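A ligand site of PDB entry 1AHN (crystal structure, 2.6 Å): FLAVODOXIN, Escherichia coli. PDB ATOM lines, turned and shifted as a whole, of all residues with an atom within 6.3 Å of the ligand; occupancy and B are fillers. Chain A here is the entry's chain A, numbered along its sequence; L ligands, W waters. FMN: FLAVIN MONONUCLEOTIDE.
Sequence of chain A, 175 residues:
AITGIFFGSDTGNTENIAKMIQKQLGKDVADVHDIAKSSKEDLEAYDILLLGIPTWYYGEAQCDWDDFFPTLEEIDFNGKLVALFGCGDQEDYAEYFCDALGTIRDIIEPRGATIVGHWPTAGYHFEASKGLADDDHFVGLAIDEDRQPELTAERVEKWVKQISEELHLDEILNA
The backbone carbonyl oxygen of Thr 55 sits at hydrogen-bond distance from an oxygen (O2') of the ligand (2.6 Å).
OD2 of Asp 146 sits at hydrogen-bond distance from O3' of the ligand.
The indole nitrogen of Trp 56 lies within hydrogen-bond range of an oxygen (O2P) of the ligand (2.7 Å).
O1P of the ligand is in hydrogen-bond range of N of Thr 11 (3.0 Å).
O1P of the ligand sits at hydrogen-bond distance from OG1 of Thr 11, 2.7 Å away.
The backbone NH of Thr 14 lies within hydrogen-bond range of an oxygen (O3P) of the ligand (2.8 Å).
OG1 of Thr 14 sits at hydrogen-bond distance from O3P of the ligand, 3.0 Å away.
O3P of the ligand is in hydrogen-bond range of OG of Ser 9, at 2.8 Å.
The backbone NH (N) of Asn 13 is in hydrogen-bond range of an oxygen (O1P) of the ligand (2.8 Å).
O4' of the ligand sits at hydrogen-bond distance from OD1 of Asn 13, at 2.9 Å.
The backbone NH (N) of Asp 10 lies within hydrogen-bond range of an oxygen (O2P) of the ligand, 2.9 Å away.
The backbone NH (N) of Gly 59 sits at hydrogen-bond distance from an oxygen (O4) of the ligand, 3.0 Å away.
The backbone NH (N) of Asp 89 lies within hydrogen-bond range of an oxygen (O2) of the ligand.
N of Gly 12 is in hydrogen-bond range of O1P of the ligand (3.1 Å).
The backbone NH (N) of Cys 98 is in hydrogen-bond range of an oxygen (O2) of the ligand, at 3.1 Å.
N of Tyr 58 is in hydrogen-bond range of O4 of the ligand, 3.2 Å away.
N5 of the ligand sits at hydrogen-bond distance from N of Tyr 57 (3.3 Å).
O of Tyr 96 sits at hydrogen-bond distance from N3 of the ligand, at 3.4 Å.
The backbone NH (N) of Thr 55 lies within hydrogen-bond range of the backbone carbonyl oxygen (O) of Cys 87 (3.3 Å).
The side-chain hydroxyl (OG1) of Thr 55 lies within hydrogen-bond range of the backbone NH (N) of Asp 99 (3.2 Å).
The backbone NH (N) of Asp 146 lies within hydrogen-bond range of the side-chain carboxylate (OD1) of Asp 144 (3.1 Å).
OG of Ser 9 lies close to N of Gly 12, at 3.3 Å.
OG of Ser 9 lies within hydrogen-bond range of N of Glu 15.
The side-chain amide nitrogen (NE2) of Gln 62 sits at hydrogen-bond distance from the backbone carbonyl oxygen (O) of Ser 9 (3.4 Å).
The side-chain amide nitrogen (NE2) of Gln 62 lies within hydrogen-bond range of the side-chain carboxylate (OD1) of Asp 10, at 2.8 Å.
N of Gly 88 sits at hydrogen-bond distance from O of Ile 143, 2.7 Å away.
Residues that only touch the ligand: Pro 54 (3.4 Å), Cys 87 (3.2 Å), Gly 88 (3.1 Å), Tyr 93 (3.2 Å) and Phe 97 (3.4 Å).
Within 4 Å of the ligand: Ser 9, Asp 10, Thr 11, Gly 12, Asn 13, Thr 14, Pro 54, Thr 55, Trp 56, Tyr 57, Tyr 58, Gly 59, Cys 87, Gly 88, Asp 89, Tyr 93, Tyr 96, Phe 97, Cys 98 and Asp 146.
The nearest printed residue that does not touch the ligand is Gly 8 (4.2 Å).
Water W2 bridges an oxygen (O3') of the ligand (2.6 Å) and the side-chain hydroxyl (OG1) of Thr 11 (2.9 Å).
Water W3 lies within hydrogen-bond range of the backbone carbonyl oxygen (O) of Gly 88 (2.7 Å), the backbone NH (N) of Glu 145 (2.7 Å), an oxygen (O4') of the ligand (2.9 Å) and the side-chain carboxylate (OD2) of Asp 146 (3.1 Å).
Water W4 lies within hydrogen-bond range of OD2 of Asp 146 and OD2 of Asp 89.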
ATOM      1  N   GLY A   8     -17.265  -3.496   4.844  1.00  0.00           N
ATOM      2  CA  GLY A   8     -16.365  -4.623   4.746  1.00  0.00           C
ATOM      3  C   GLY A   8     -16.933  -5.506   5.845  1.00  0.00           C
ATOM      4  O   GLY A   8     -17.427  -4.995   6.868  1.00  0.00           O
ATOM      5  N   SER A   9     -16.990  -6.814   5.633  1.00  0.00           N
ATOM      6  CA  SER A   9     -17.532  -7.676   6.658  1.00  0.00           C
ATOM      7  C   SER A   9     -16.950  -9.048   6.432  1.00  0.00           C
ATOM      8  O   SER A   9     -16.815  -9.474   5.288  1.00  0.00           O
ATOM      9  CB  SER A   9     -19.055  -7.729   6.534  1.00  0.00           C
ATOM     10  OG  SER A   9     -19.629  -8.319   7.673  1.00  0.00           O
ATOM     11  N   ASP A  10     -16.546  -9.714   7.498  1.00  0.00           N
ATOM     12  CA  ASP A  10     -15.982 -11.046   7.337  1.00  0.00           C
ATOM     13  C   ASP A  10     -16.850 -12.161   7.897  1.00  0.00           C
ATOM     14  O   ASP A  10     -16.942 -13.224   7.295  1.00  0.00           O
ATOM     15  CB  ASP A  10     -14.522 -11.103   7.796  1.00  0.00           C
ATOM     16  CG  ASP A  10     -13.551 -10.619   6.708  1.00  0.00           C
ATOM     17  OD1 ASP A  10     -13.845 -10.828   5.516  1.00  0.00           O
ATOM     18  OD2 ASP A  10     -12.485 -10.045   7.033  1.00  0.00           O
ATOM     19  N   THR A  11     -17.549 -11.894   9.001  1.00  0.00           N
ATOM     20  CA  THR A  11     -18.456 -12.874   9.607  1.00  0.00           C
ATOM     21  C   THR A  11     -19.891 -12.346   9.635  1.00  0.00           C
ATOM     22  O   THR A  11     -20.729 -12.798  10.436  1.00  0.00           O
ATOM     23  CB  THR A  11     -18.032 -13.280  11.033  1.00  0.00           C
ATOM     24  OG1 THR A  11     -17.512 -12.145  11.728  1.00  0.00           O
ATOM     25  CG2 THR A  11     -16.960 -14.366  10.972  1.00  0.00           C
ATOM     26  N   GLY A  12     -20.132 -11.335   8.802  1.00  0.00           N
ATOM     27  CA  GLY A  12     -21.442 -10.727   8.635  1.00  0.00           C
ATOM     28  C   GLY A  12     -21.919  -9.570   9.494  1.00  0.00           C
ATOM     29  O   GLY A  12     -22.857  -8.851   9.104  1.00  0.00           O
ATOM     30  N   ASN A  13     -21.265  -9.286  10.609  1.00  0.00           N
ATOM     31  CA  ASN A  13     -21.754  -8.235  11.478  1.00  0.00           C
ATOM     32  C   ASN A  13     -21.828  -6.860  10.840  1.00  0.00           C
ATOM     33  O   ASN A  13     -22.920  -6.286  10.719  1.00  0.00           O
ATOM     34  CB  ASN A  13     -20.959  -8.220  12.775  1.00  0.00           C
ATOM     35  CG  ASN A  13     -21.186  -9.476  13.599  1.00  0.00           C
ATOM     36  OD1 ASN A  13     -20.254 -10.052  14.138  1.00  0.00           O
ATOM     37  ND2 ASN A  13     -22.429  -9.914  13.702  1.00  0.00           N
ATOM     38  N   THR A  14     -20.704  -6.341  10.369  1.00  0.00           N
ATOM     39  CA  THR A  14     -20.726  -5.025   9.778  1.00  0.00           C
ATOM     40  C   THR A  14     -21.711  -4.962   8.603  1.00  0.00           C
ATOM     41  O   THR A  14     -22.451  -3.996   8.464  1.00  0.00           O
ATOM     42  CB  THR A  14     -19.328  -4.579   9.379  1.00  0.00           C
ATOM     43  OG1 THR A  14     -18.457  -4.687  10.520  1.00  0.00           O
ATOM     44  CG2 THR A  14     -19.352  -3.160   8.902  1.00  0.00           C
ATOM     45  N   GLU A  15     -21.804  -6.046   7.841  1.00  0.00           N
ATOM     46  CA  GLU A  15     -22.723  -6.106   6.715  1.00  0.00           C
ATOM     47  C   GLU A  15     -24.177  -5.897   7.193  1.00  0.00           C
ATOM     48  O   GLU A  15     -24.968  -5.269   6.504  1.00  0.00           O
ATOM     49  CB  GLU A  15     -22.551  -7.449   6.034  1.00  0.00           C
ATOM     50  CG  GLU A  15     -23.361  -7.648   4.788  1.00  0.00           C
ATOM     51  CD  GLU A  15     -23.028  -8.960   4.099  1.00  0.00           C
ATOM     52  OE1 GLU A  15     -21.848  -9.380   4.170  1.00  0.00           O
ATOM     53  OE2 GLU A  15     -23.935  -9.575   3.485  1.00  0.00           O
ATOM     54  N   PRO A  54     -14.883  -3.274  10.474  1.00  0.00           N
ATOM     55  CA  PRO A  54     -14.711  -4.008  11.721  1.00  0.00           C
ATOM     56  C   PRO A  54     -13.205  -4.234  11.857  1.00  0.00           C
ATOM     57  O   PRO A  54     -12.505  -4.296  10.845  1.00  0.00           O
ATOM     58  CB  PRO A  54     -15.445  -5.308  11.453  1.00  0.00           C
ATOM     59  CG  PRO A  54     -15.207  -5.525  10.010  1.00  0.00           C
ATOM     60  CD  PRO A  54     -15.450  -4.162   9.436  1.00  0.00           C
ATOM     61  N   THR A  55     -12.737  -4.301  13.096  1.00  0.00           N
ATOM     62  CA  THR A  55     -11.335  -4.491  13.414  1.00  0.00           C
ATOM     63  C   THR A  55     -11.033  -5.995  13.561  1.00  0.00           C
ATOM     64  O   THR A  55     -11.719  -6.734  14.260  1.00  0.00           O
ATOM     65  CB  THR A  55     -10.992  -3.705  14.695  1.00  0.00           C
ATOM     66  OG1 THR A  55     -11.328  -2.331  14.481  1.00  0.00           O
ATOM     67  CG2 THR A  55      -9.499  -3.793  15.016  1.00  0.00           C
ATOM     68  N   TRP A  56      -9.968  -6.436  12.922  1.00  0.00           N
ATOM     69  CA  TRP A  56      -9.620  -7.833  12.929  1.00  0.00           C
ATOM     70  C   TRP A  56      -8.177  -8.072  13.344  1.00  0.00           C
ATOM     71  O   TRP A  56      -7.321  -7.187  13.216  1.00  0.00           O
ATOM     72  CB  TRP A  56      -9.883  -8.459  11.544  1.00  0.00           C
ATOM     73  CG  TRP A  56     -11.311  -8.918  11.333  1.00  0.00           C
ATOM     74  CD1 TRP A  56     -12.334  -8.231  10.713  1.00  0.00           C
ATOM     75  CD2 TRP A  56     -11.881 -10.143  11.798  1.00  0.00           C
ATOM     76  NE1 TRP A  56     -13.503  -8.956  10.777  1.00  0.00           N
ATOM     77  CE2 TRP A  56     -13.248 -10.135  11.435  1.00  0.00           C
ATOM     78  CE3 TRP A  56     -11.368 -11.249  12.478  1.00  0.00           C
ATOM     79  CZ2 TRP A  56     -14.098 -11.181  11.738  1.00  0.00           C
ATOM     80  CZ3 TRP A  56     -12.215 -12.286  12.785  1.00  0.00           C
ATOM     81  CH2 TRP A  56     -13.575 -12.248  12.406  1.00  0.00           C
ATOM     82  N   TYR A  57      -7.943  -9.264  13.883  1.00  0.00           N
ATOM     83  CA  TYR A  57      -6.639  -9.712  14.324  1.00  0.00           C
ATOM     84  C   TYR A  57      -5.671  -8.728  14.888  1.00  0.00           C
ATOM     85  O   TYR A  57      -4.617  -8.481  14.309  1.00  0.00           O
ATOM     86  CB  TYR A  57      -5.894 -10.441  13.219  1.00  0.00           C
ATOM     87  CG  TYR A  57      -6.733 -10.916  12.096  1.00  0.00           C
ATOM     88  CD1 TYR A  57      -7.382 -12.133  12.161  1.00  0.00           C
ATOM     89  CD2 TYR A  57      -6.809 -10.182  10.914  1.00  0.00           C
ATOM     90  CE1 TYR A  57      -8.064 -12.622  11.078  1.00  0.00           C
ATOM     91  CE2 TYR A  57      -7.473 -10.657   9.839  1.00  0.00           C
ATOM     92  CZ  TYR A  57      -8.093 -11.879   9.921  1.00  0.00           C
ATOM     93  OH  TYR A  57      -8.622 -12.396   8.792  1.00  0.00           O
ATOM     94  N   TYR A  58      -6.033  -8.163  16.030  1.00  0.00           N
ATOM     95  CA  TYR A  58      -5.152  -7.247  16.726  1.00  0.00           C
ATOM     96  C   TYR A  58      -4.902  -5.829  16.134  1.00  0.00           C
ATOM     97  O   TYR A  58      -3.756  -5.393  15.949  1.00  0.00           O
ATOM     98  CB  TYR A  58      -3.850  -7.989  17.023  1.00  0.00           C
ATOM     99  CG  TYR A  58      -4.072  -9.497  17.258  1.00  0.00           C
ATOM    100  CD1 TYR A  58      -4.774  -9.956  18.386  1.00  0.00           C
ATOM    101  CD2 TYR A  58      -3.579 -10.439  16.356  1.00  0.00           C
ATOM    102  CE1 TYR A  58      -4.974 -11.316  18.616  1.00  0.00           C
ATOM    103  CE2 TYR A  58      -3.767 -11.805  16.569  1.00  0.00           C
ATOM    104  CZ  TYR A  58      -4.464 -12.247  17.705  1.00  0.00           C
ATOM    105  OH  TYR A  58      -4.630 -13.588  17.948  1.00  0.00           O
ATOM    106  N   GLY A  59      -5.995  -5.079  15.941  1.00  0.00           N
ATOM    107  CA  GLY A  59      -5.863  -3.732  15.412  1.00  0.00           C
ATOM    108  C   GLY A  59      -5.866  -3.621  13.901  1.00  0.00           C
ATOM    109  O   GLY A  59      -6.053  -2.533  13.363  1.00  0.00           O
ATOM    110  N   GLU A  60      -5.683  -4.740  13.205  1.00  0.00           N
ATOM    111  CA  GLU A  60      -5.664  -4.750  11.739  1.00  0.00           C
ATOM    112  C   GLU A  60      -7.011  -4.403  11.133  1.00  0.00           C
ATOM    113  O   GLU A  60      -8.033  -4.350  11.831  1.00  0.00           O
ATOM    114  CB  GLU A  60      -5.219  -6.121  11.199  1.00  0.00           C
ATOM    115  CG  GLU A  60      -3.790  -6.498  11.553  1.00  0.00           C
ATOM    116  CD  GLU A  60      -2.941  -5.272  11.908  1.00  0.00           C
ATOM    117  OE1 GLU A  60      -2.518  -4.543  10.979  1.00  0.00           O
ATOM    118  OE2 GLU A  60      -2.708  -5.047  13.124  1.00  0.00           O
ATOM    119  N   GLN A  62     -10.177  -5.146   8.425  1.00  0.00           N
ATOM    120  CA  GLN A  62     -10.857  -6.220   7.712  1.00  0.00           C
ATOM    121  C   GLN A  62     -10.148  -6.307   6.365  1.00  0.00           C
ATOM    122  O   GLN A  62      -9.925  -5.290   5.715  1.00  0.00           O
ATOM    123  CB  GLN A  62     -12.309  -5.832   7.550  1.00  0.00           C
ATOM    124  CG  GLN A  62     -13.186  -6.927   7.067  1.00  0.00           C
ATOM    125  CD  GLN A  62     -13.312  -6.901   5.581  1.00  0.00           C
ATOM    126  OE1 GLN A  62     -13.074  -5.885   4.948  1.00  0.00           O
ATOM    127  NE2 GLN A  62     -13.711  -8.029   5.012  1.00  0.00           N
ATOM    128  N   CYS A  87     -17.451  -2.665  13.661  1.00  0.00           N
ATOM    129  CA  CYS A  87     -17.778  -3.576  14.739  1.00  0.00           C
ATOM    130  C   CYS A  87     -16.503  -3.902  15.451  1.00  0.00           C
ATOM    131  O   CYS A  87     -15.419  -3.743  14.871  1.00  0.00           O
ATOM    132  CB  CYS A  87     -18.440  -4.860  14.201  1.00  0.00           C
ATOM    133  SG  CYS A  87     -19.982  -4.570  13.311  1.00  0.00           S
ATOM    134  N   GLY A  88     -16.623  -4.312  16.709  1.00  0.00           N
ATOM    135  CA  GLY A  88     -15.450  -4.674  17.496  1.00  0.00           C
ATOM    136  C   GLY A  88     -15.852  -5.568  18.646  1.00  0.00           C
ATOM    137  O   GLY A  88     -17.049  -5.861  18.848  1.00  0.00           O
ATOM    138  N   ASP A  89     -14.853  -6.009  19.384  1.00  0.00           N
ATOM    139  CA  ASP A  89     -15.067  -6.885  20.538  1.00  0.00           C
ATOM    140  C   ASP A  89     -14.261  -6.244  21.645  1.00  0.00           C
ATOM    141  O   ASP A  89     -13.026  -6.320  21.669  1.00  0.00           O
ATOM    142  CB  ASP A  89     -14.563  -8.298  20.229  1.00  0.00           C
ATOM    143  CG  ASP A  89     -14.864  -9.285  21.351  1.00  0.00           C
ATOM    144  OD1 ASP A  89     -15.155  -8.848  22.485  1.00  0.00           O
ATOM    145  OD2 ASP A  89     -14.807 -10.511  21.104  1.00  0.00           O
ATOM    146  N   GLN A  90     -14.972  -5.602  22.568  1.00  0.00           N
ATOM    147  CA  GLN A  90     -14.377  -4.875  23.680  1.00  0.00           C
ATOM    148  C   GLN A  90     -13.959  -5.727  24.878  1.00  0.00           C
ATOM    149  O   GLN A  90     -13.392  -5.191  25.838  1.00  0.00           O
ATOM    150  CB  GLN A  90     -15.336  -3.779  24.137  1.00  0.00           C
ATOM    151  CG  GLN A  90     -16.574  -4.360  24.739  1.00  0.00           C
ATOM    152  CD  GLN A  90     -17.655  -3.356  24.988  1.00  0.00           C
ATOM    153  OE1 GLN A  90     -17.678  -2.710  26.030  1.00  0.00           O
ATOM    154  NE2 GLN A  90     -18.579  -3.245  24.048  1.00  0.00           N
ATOM    155  N   TYR A  93     -10.763  -8.404  22.836  1.00  0.00           N
ATOM    156  CA  TYR A  93      -9.825  -7.583  22.076  1.00  0.00           C
ATOM    157  C   TYR A  93     -10.012  -6.131  22.532  1.00  0.00           C
ATOM    158  O   TYR A  93      -9.888  -5.183  21.751  1.00  0.00           O
ATOM    159  CB  TYR A  93     -10.082  -7.761  20.579  1.00  0.00           C
ATOM    160  CG  TYR A  93      -9.980  -9.232  20.114  1.00  0.00           C
ATOM    161  CD1 TYR A  93      -8.730  -9.811  19.829  1.00  0.00           C
ATOM    162  CD2 TYR A  93     -11.120 -10.035  20.024  1.00  0.00           C
ATOM    163  CE1 TYR A  93      -8.632 -11.156  19.480  1.00  0.00           C
ATOM    164  CE2 TYR A  93     -11.022 -11.381  19.675  1.00  0.00           C
ATOM    165  CZ  TYR A  93      -9.778 -11.928  19.421  1.00  0.00           C
ATOM    166  OH  TYR A  93      -9.679 -13.276  19.166  1.00  0.00           O
ATOM    167  N   ALA A  94     -10.204  -5.984  23.841  1.00  0.00           N
ATOM    168  CA  ALA A  94     -10.430  -4.711  24.506  1.00  0.00           C
ATOM    169  C   ALA A  94      -9.319  -3.759  24.255  1.00  0.00           C
ATOM    170  O   ALA A  94      -9.506  -2.550  24.377  1.00  0.00           O
ATOM    171  CB  ALA A  94     -10.555  -4.899  26.006  1.00  0.00           C
ATOM    172  N   TYR A  96      -7.791  -3.240  21.437  1.00  0.00           N
ATOM    173  CA  TYR A  96      -7.718  -2.802  20.038  1.00  0.00           C
ATOM    174  C   TYR A  96      -9.115  -2.462  19.605  1.00  0.00           C
ATOM    175  O   TYR A  96      -9.379  -2.344  18.411  1.00  0.00           O
ATOM    176  CB  TYR A  96      -7.222  -3.903  19.105  1.00  0.00           C
ATOM    177  CG  TYR A  96      -6.150  -4.769  19.667  1.00  0.00           C
ATOM    178  CD1 TYR A  96      -4.830  -4.326  19.716  1.00  0.00           C
ATOM    179  CD2 TYR A  96      -6.441  -5.996  20.222  1.00  0.00           C
ATOM    180  CE1 TYR A  96      -3.823  -5.104  20.298  1.00  0.00           C
ATOM    181  CE2 TYR A  96      -5.441  -6.776  20.810  1.00  0.00           C
ATOM    182  CZ  TYR A  96      -4.148  -6.320  20.848  1.00  0.00           C
ATOM    183  OH  TYR A  96      -3.186  -7.051  21.495  1.00  0.00           O
ATOM    184  N   PHE A  97     -10.015  -2.294  20.577  1.00  0.00           N
ATOM    185  CA  PHE A  97     -11.429  -2.037  20.292  1.00  0.00           C
ATOM    186  C   PHE A  97     -11.738  -0.988  19.218  1.00  0.00           C
ATOM    187  O   PHE A  97     -11.744   0.210  19.472  1.00  0.00           O
ATOM    188  CB  PHE A  97     -12.190  -1.712  21.584  1.00  0.00           C
ATOM    189  CG  PHE A  97     -13.671  -1.649  21.395  1.00  0.00           C
ATOM    190  CD1 PHE A  97     -14.382  -2.789  21.049  1.00  0.00           C
ATOM    191  CD2 PHE A  97     -14.363  -0.449  21.518  1.00  0.00           C
ATOM    192  CE1 PHE A  97     -15.757  -2.735  20.826  1.00  0.00           C
ATOM    193  CE2 PHE A  97     -15.737  -0.387  21.299  1.00  0.00           C
ATOM    194  CZ  PHE A  97     -16.436  -1.539  20.949  1.00  0.00           C
ATOM    195  N   CYS A  98     -12.042  -1.475  18.031  1.00  0.00           N
ATOM    196  CA  CYS A  98     -12.384  -0.612  16.909  1.00  0.00           C
ATOM    197  C   CYS A  98     -11.255   0.286  16.419  1.00  0.00           C
ATOM    198  O   CYS A  98     -11.512   1.380  15.926  1.00  0.00           O
ATOM    199  CB  CYS A  98     -13.653   0.186  17.204  1.00  0.00           C
ATOM    200  SG  CYS A  98     -15.147  -0.839  17.429  1.00  0.00           S
ATOM    201  N   ASP A  99     -10.029  -0.214  16.464  1.00  0.00           N
ATOM    202  CA  ASP A  99      -8.879   0.564  15.972  1.00  0.00           C
ATOM    203  C   ASP A  99      -9.047   0.861  14.496  1.00  0.00           C
ATOM    204  O   ASP A  99      -8.720   1.956  14.046  1.00  0.00           O
ATOM    205  CB  ASP A  99      -7.570  -0.203  16.179  1.00  0.00           C
ATOM    206  CG  ASP A  99      -7.138  -0.254  17.629  1.00  0.00           C
ATOM    207  OD1 ASP A  99      -7.903   0.209  18.499  1.00  0.00           O
ATOM    208  OD2 ASP A  99      -6.030  -0.743  17.912  1.00  0.00           O
ATOM    209  N   ILE A 143     -19.815  -0.721  17.111  1.00  0.00           N
ATOM    210  CA  ILE A 143     -20.829  -1.727  17.418  1.00  0.00           C
ATOM    211  C   ILE A 143     -20.135  -2.997  17.901  1.00  0.00           C
ATOM    212  O   ILE A 143     -19.145  -3.455  17.310  1.00  0.00           O
ATOM    213  CB  ILE A 143     -21.696  -2.067  16.183  1.00  0.00           C
ATOM    214  CG1 ILE A 143     -22.543  -0.863  15.771  1.00  0.00           C
ATOM    215  CG2 ILE A 143     -22.619  -3.238  16.497  1.00  0.00           C
ATOM    216  CD1 ILE A 143     -23.780  -0.690  16.632  1.00  0.00           C
ATOM    217  N   ASP A 144     -20.649  -3.546  18.996  1.00  0.00           N
ATOM    218  CA  ASP A 144     -20.095  -4.770  19.527  1.00  0.00           C
ATOM    219  C   ASP A 144     -21.232  -5.779  19.566  1.00  0.00           C
ATOM    220  O   ASP A 144     -22.033  -5.824  20.499  1.00  0.00           O
ATOM    221  CB  ASP A 144     -19.489  -4.524  20.918  1.00  0.00           C
ATOM    222  CG  ASP A 144     -18.691  -5.731  21.427  1.00  0.00           C
ATOM    223  OD1 ASP A 144     -18.949  -6.855  20.960  1.00  0.00           O
ATOM    224  OD2 ASP A 144     -17.799  -5.549  22.286  1.00  0.00           O
ATOM    225  N   GLU A 145     -21.290  -6.578  18.504  1.00  0.00           N
ATOM    226  CA  GLU A 145     -22.301  -7.592  18.332  1.00  0.00           C
ATOM    227  C   GLU A 145     -21.897  -8.849  19.069  1.00  0.00           C
ATOM    228  O   GLU A 145     -22.700  -9.782  19.219  1.00  0.00           O
ATOM    229  CB  GLU A 145     -22.461  -7.911  16.839  1.00  0.00           C
ATOM    230  CG  GLU A 145     -23.257  -6.878  16.016  1.00  0.00           C
ATOM    231  CD  GLU A 145     -24.749  -6.869  16.361  1.00  0.00           C
ATOM    232  OE1 GLU A 145     -25.084  -6.734  17.563  1.00  0.00           O
ATOM    233  OE2 GLU A 145     -25.592  -7.023  15.425  1.00  0.00           O
ATOM    234  N   ASP A 146     -20.623  -8.912  19.451  1.00  0.00           N
ATOM    235  CA  ASP A 146     -20.096 -10.054  20.170  1.00  0.00           C
ATOM    236  C   ASP A 146     -20.464  -9.983  21.647  1.00  0.00           C
ATOM    237  O   ASP A 146     -20.826 -10.997  22.228  1.00  0.00           O
ATOM    238  CB  ASP A 146     -18.580 -10.100  20.063  1.00  0.00           C
ATOM    239  CG  ASP A 146     -18.076 -10.575  18.719  1.00  0.00           C
ATOM    240  OD1 ASP A 146     -18.387 -11.715  18.311  1.00  0.00           O
ATOM    241  OD2 ASP A 146     -17.306  -9.824  18.089  1.00  0.00           O
HETATM  242  N1  FMN L   1     -12.521  -6.641  17.388  1.00  0.00           N
HETATM  243  C2  FMN L   1     -11.867  -5.494  17.747  1.00  0.00           C
HETATM  244  O2  FMN L   1     -12.419  -4.588  18.325  1.00  0.00           O
HETATM  245  N3  FMN L   1     -10.515  -5.396  17.465  1.00  0.00           N
HETATM  246  C4  FMN L   1      -9.680  -6.479  17.224  1.00  0.00           C
HETATM  247  O4  FMN L   1      -8.413  -6.359  17.188  1.00  0.00           O
HETATM  248  C4A FMN L   1     -10.371  -7.780  16.959  1.00  0.00           C
HETATM  249  N5  FMN L   1      -9.670  -8.869  16.638  1.00  0.00           N
HETATM  250  C5A FMN L   1     -10.337 -10.010  16.296  1.00  0.00           C
HETATM  251  C6  FMN L   1      -9.620 -11.227  16.151  1.00  0.00           C
HETATM  252  C7  FMN L   1     -10.277 -12.465  16.080  1.00  0.00           C
HETATM  253  C7M FMN L   1      -9.480 -13.716  16.005  1.00  0.00           C
HETATM  254  C8  FMN L   1     -11.729 -12.475  16.063  1.00  0.00           C
HETATM  255  C8M FMN L   1     -12.589 -13.676  15.933  1.00  0.00           C
HETATM  256  C9  FMN L   1     -12.438 -11.279  16.135  1.00  0.00           C
HETATM  257  C9A FMN L   1     -11.760 -10.049  16.276  1.00  0.00           C
HETATM  258  N10 FMN L   1     -12.447  -8.906  16.641  1.00  0.00           N
HETATM  259  C10 FMN L   1     -11.822  -7.734  17.033  1.00  0.00           C
HETATM  260  C1' FMN L   1     -13.924  -8.992  16.671  1.00  0.00           C
HETATM  261  C2' FMN L   1     -14.564  -8.499  15.386  1.00  0.00           C
HETATM  262  O2' FMN L   1     -14.218  -7.253  14.790  1.00  0.00           O
HETATM  263  C3' FMN L   1     -16.045  -8.605  15.501  1.00  0.00           C
HETATM  264  O3' FMN L   1     -16.383  -9.984  15.613  1.00  0.00           O
HETATM  265  C4' FMN L   1     -16.866  -7.972  14.392  1.00  0.00           C
HETATM  266  O4' FMN L   1     -18.257  -8.031  14.729  1.00  0.00           O
HETATM  267  C5' FMN L   1     -16.662  -8.753  13.097  1.00  0.00           C
HETATM  268  O5' FMN L   1     -17.398  -8.080  12.048  1.00  0.00           O
HETATM  269  P   FMN L   1     -17.493  -8.681  10.755  1.00  0.00           P
HETATM  270  O1P FMN L   1     -18.476  -9.728  10.902  1.00  0.00           O
HETATM  271  O2P FMN L   1     -16.138  -8.932  10.231  1.00  0.00           O
HETATM  272  O3P FMN L   1     -18.234  -7.607  10.005  1.00  0.00           O
HETATM  273  O   HOH W   1     -11.954 -14.788  19.137  1.00  0.00           O
HETATM  274  O   HOH W   2     -17.078 -12.301  14.566  1.00  0.00           O
HETATM  275  O   HOH W   3     -18.865  -7.289  17.420  1.00  0.00           O
HETATM  276  O   HOH W   4     -15.240 -11.499  18.560  1.00  0.00           O
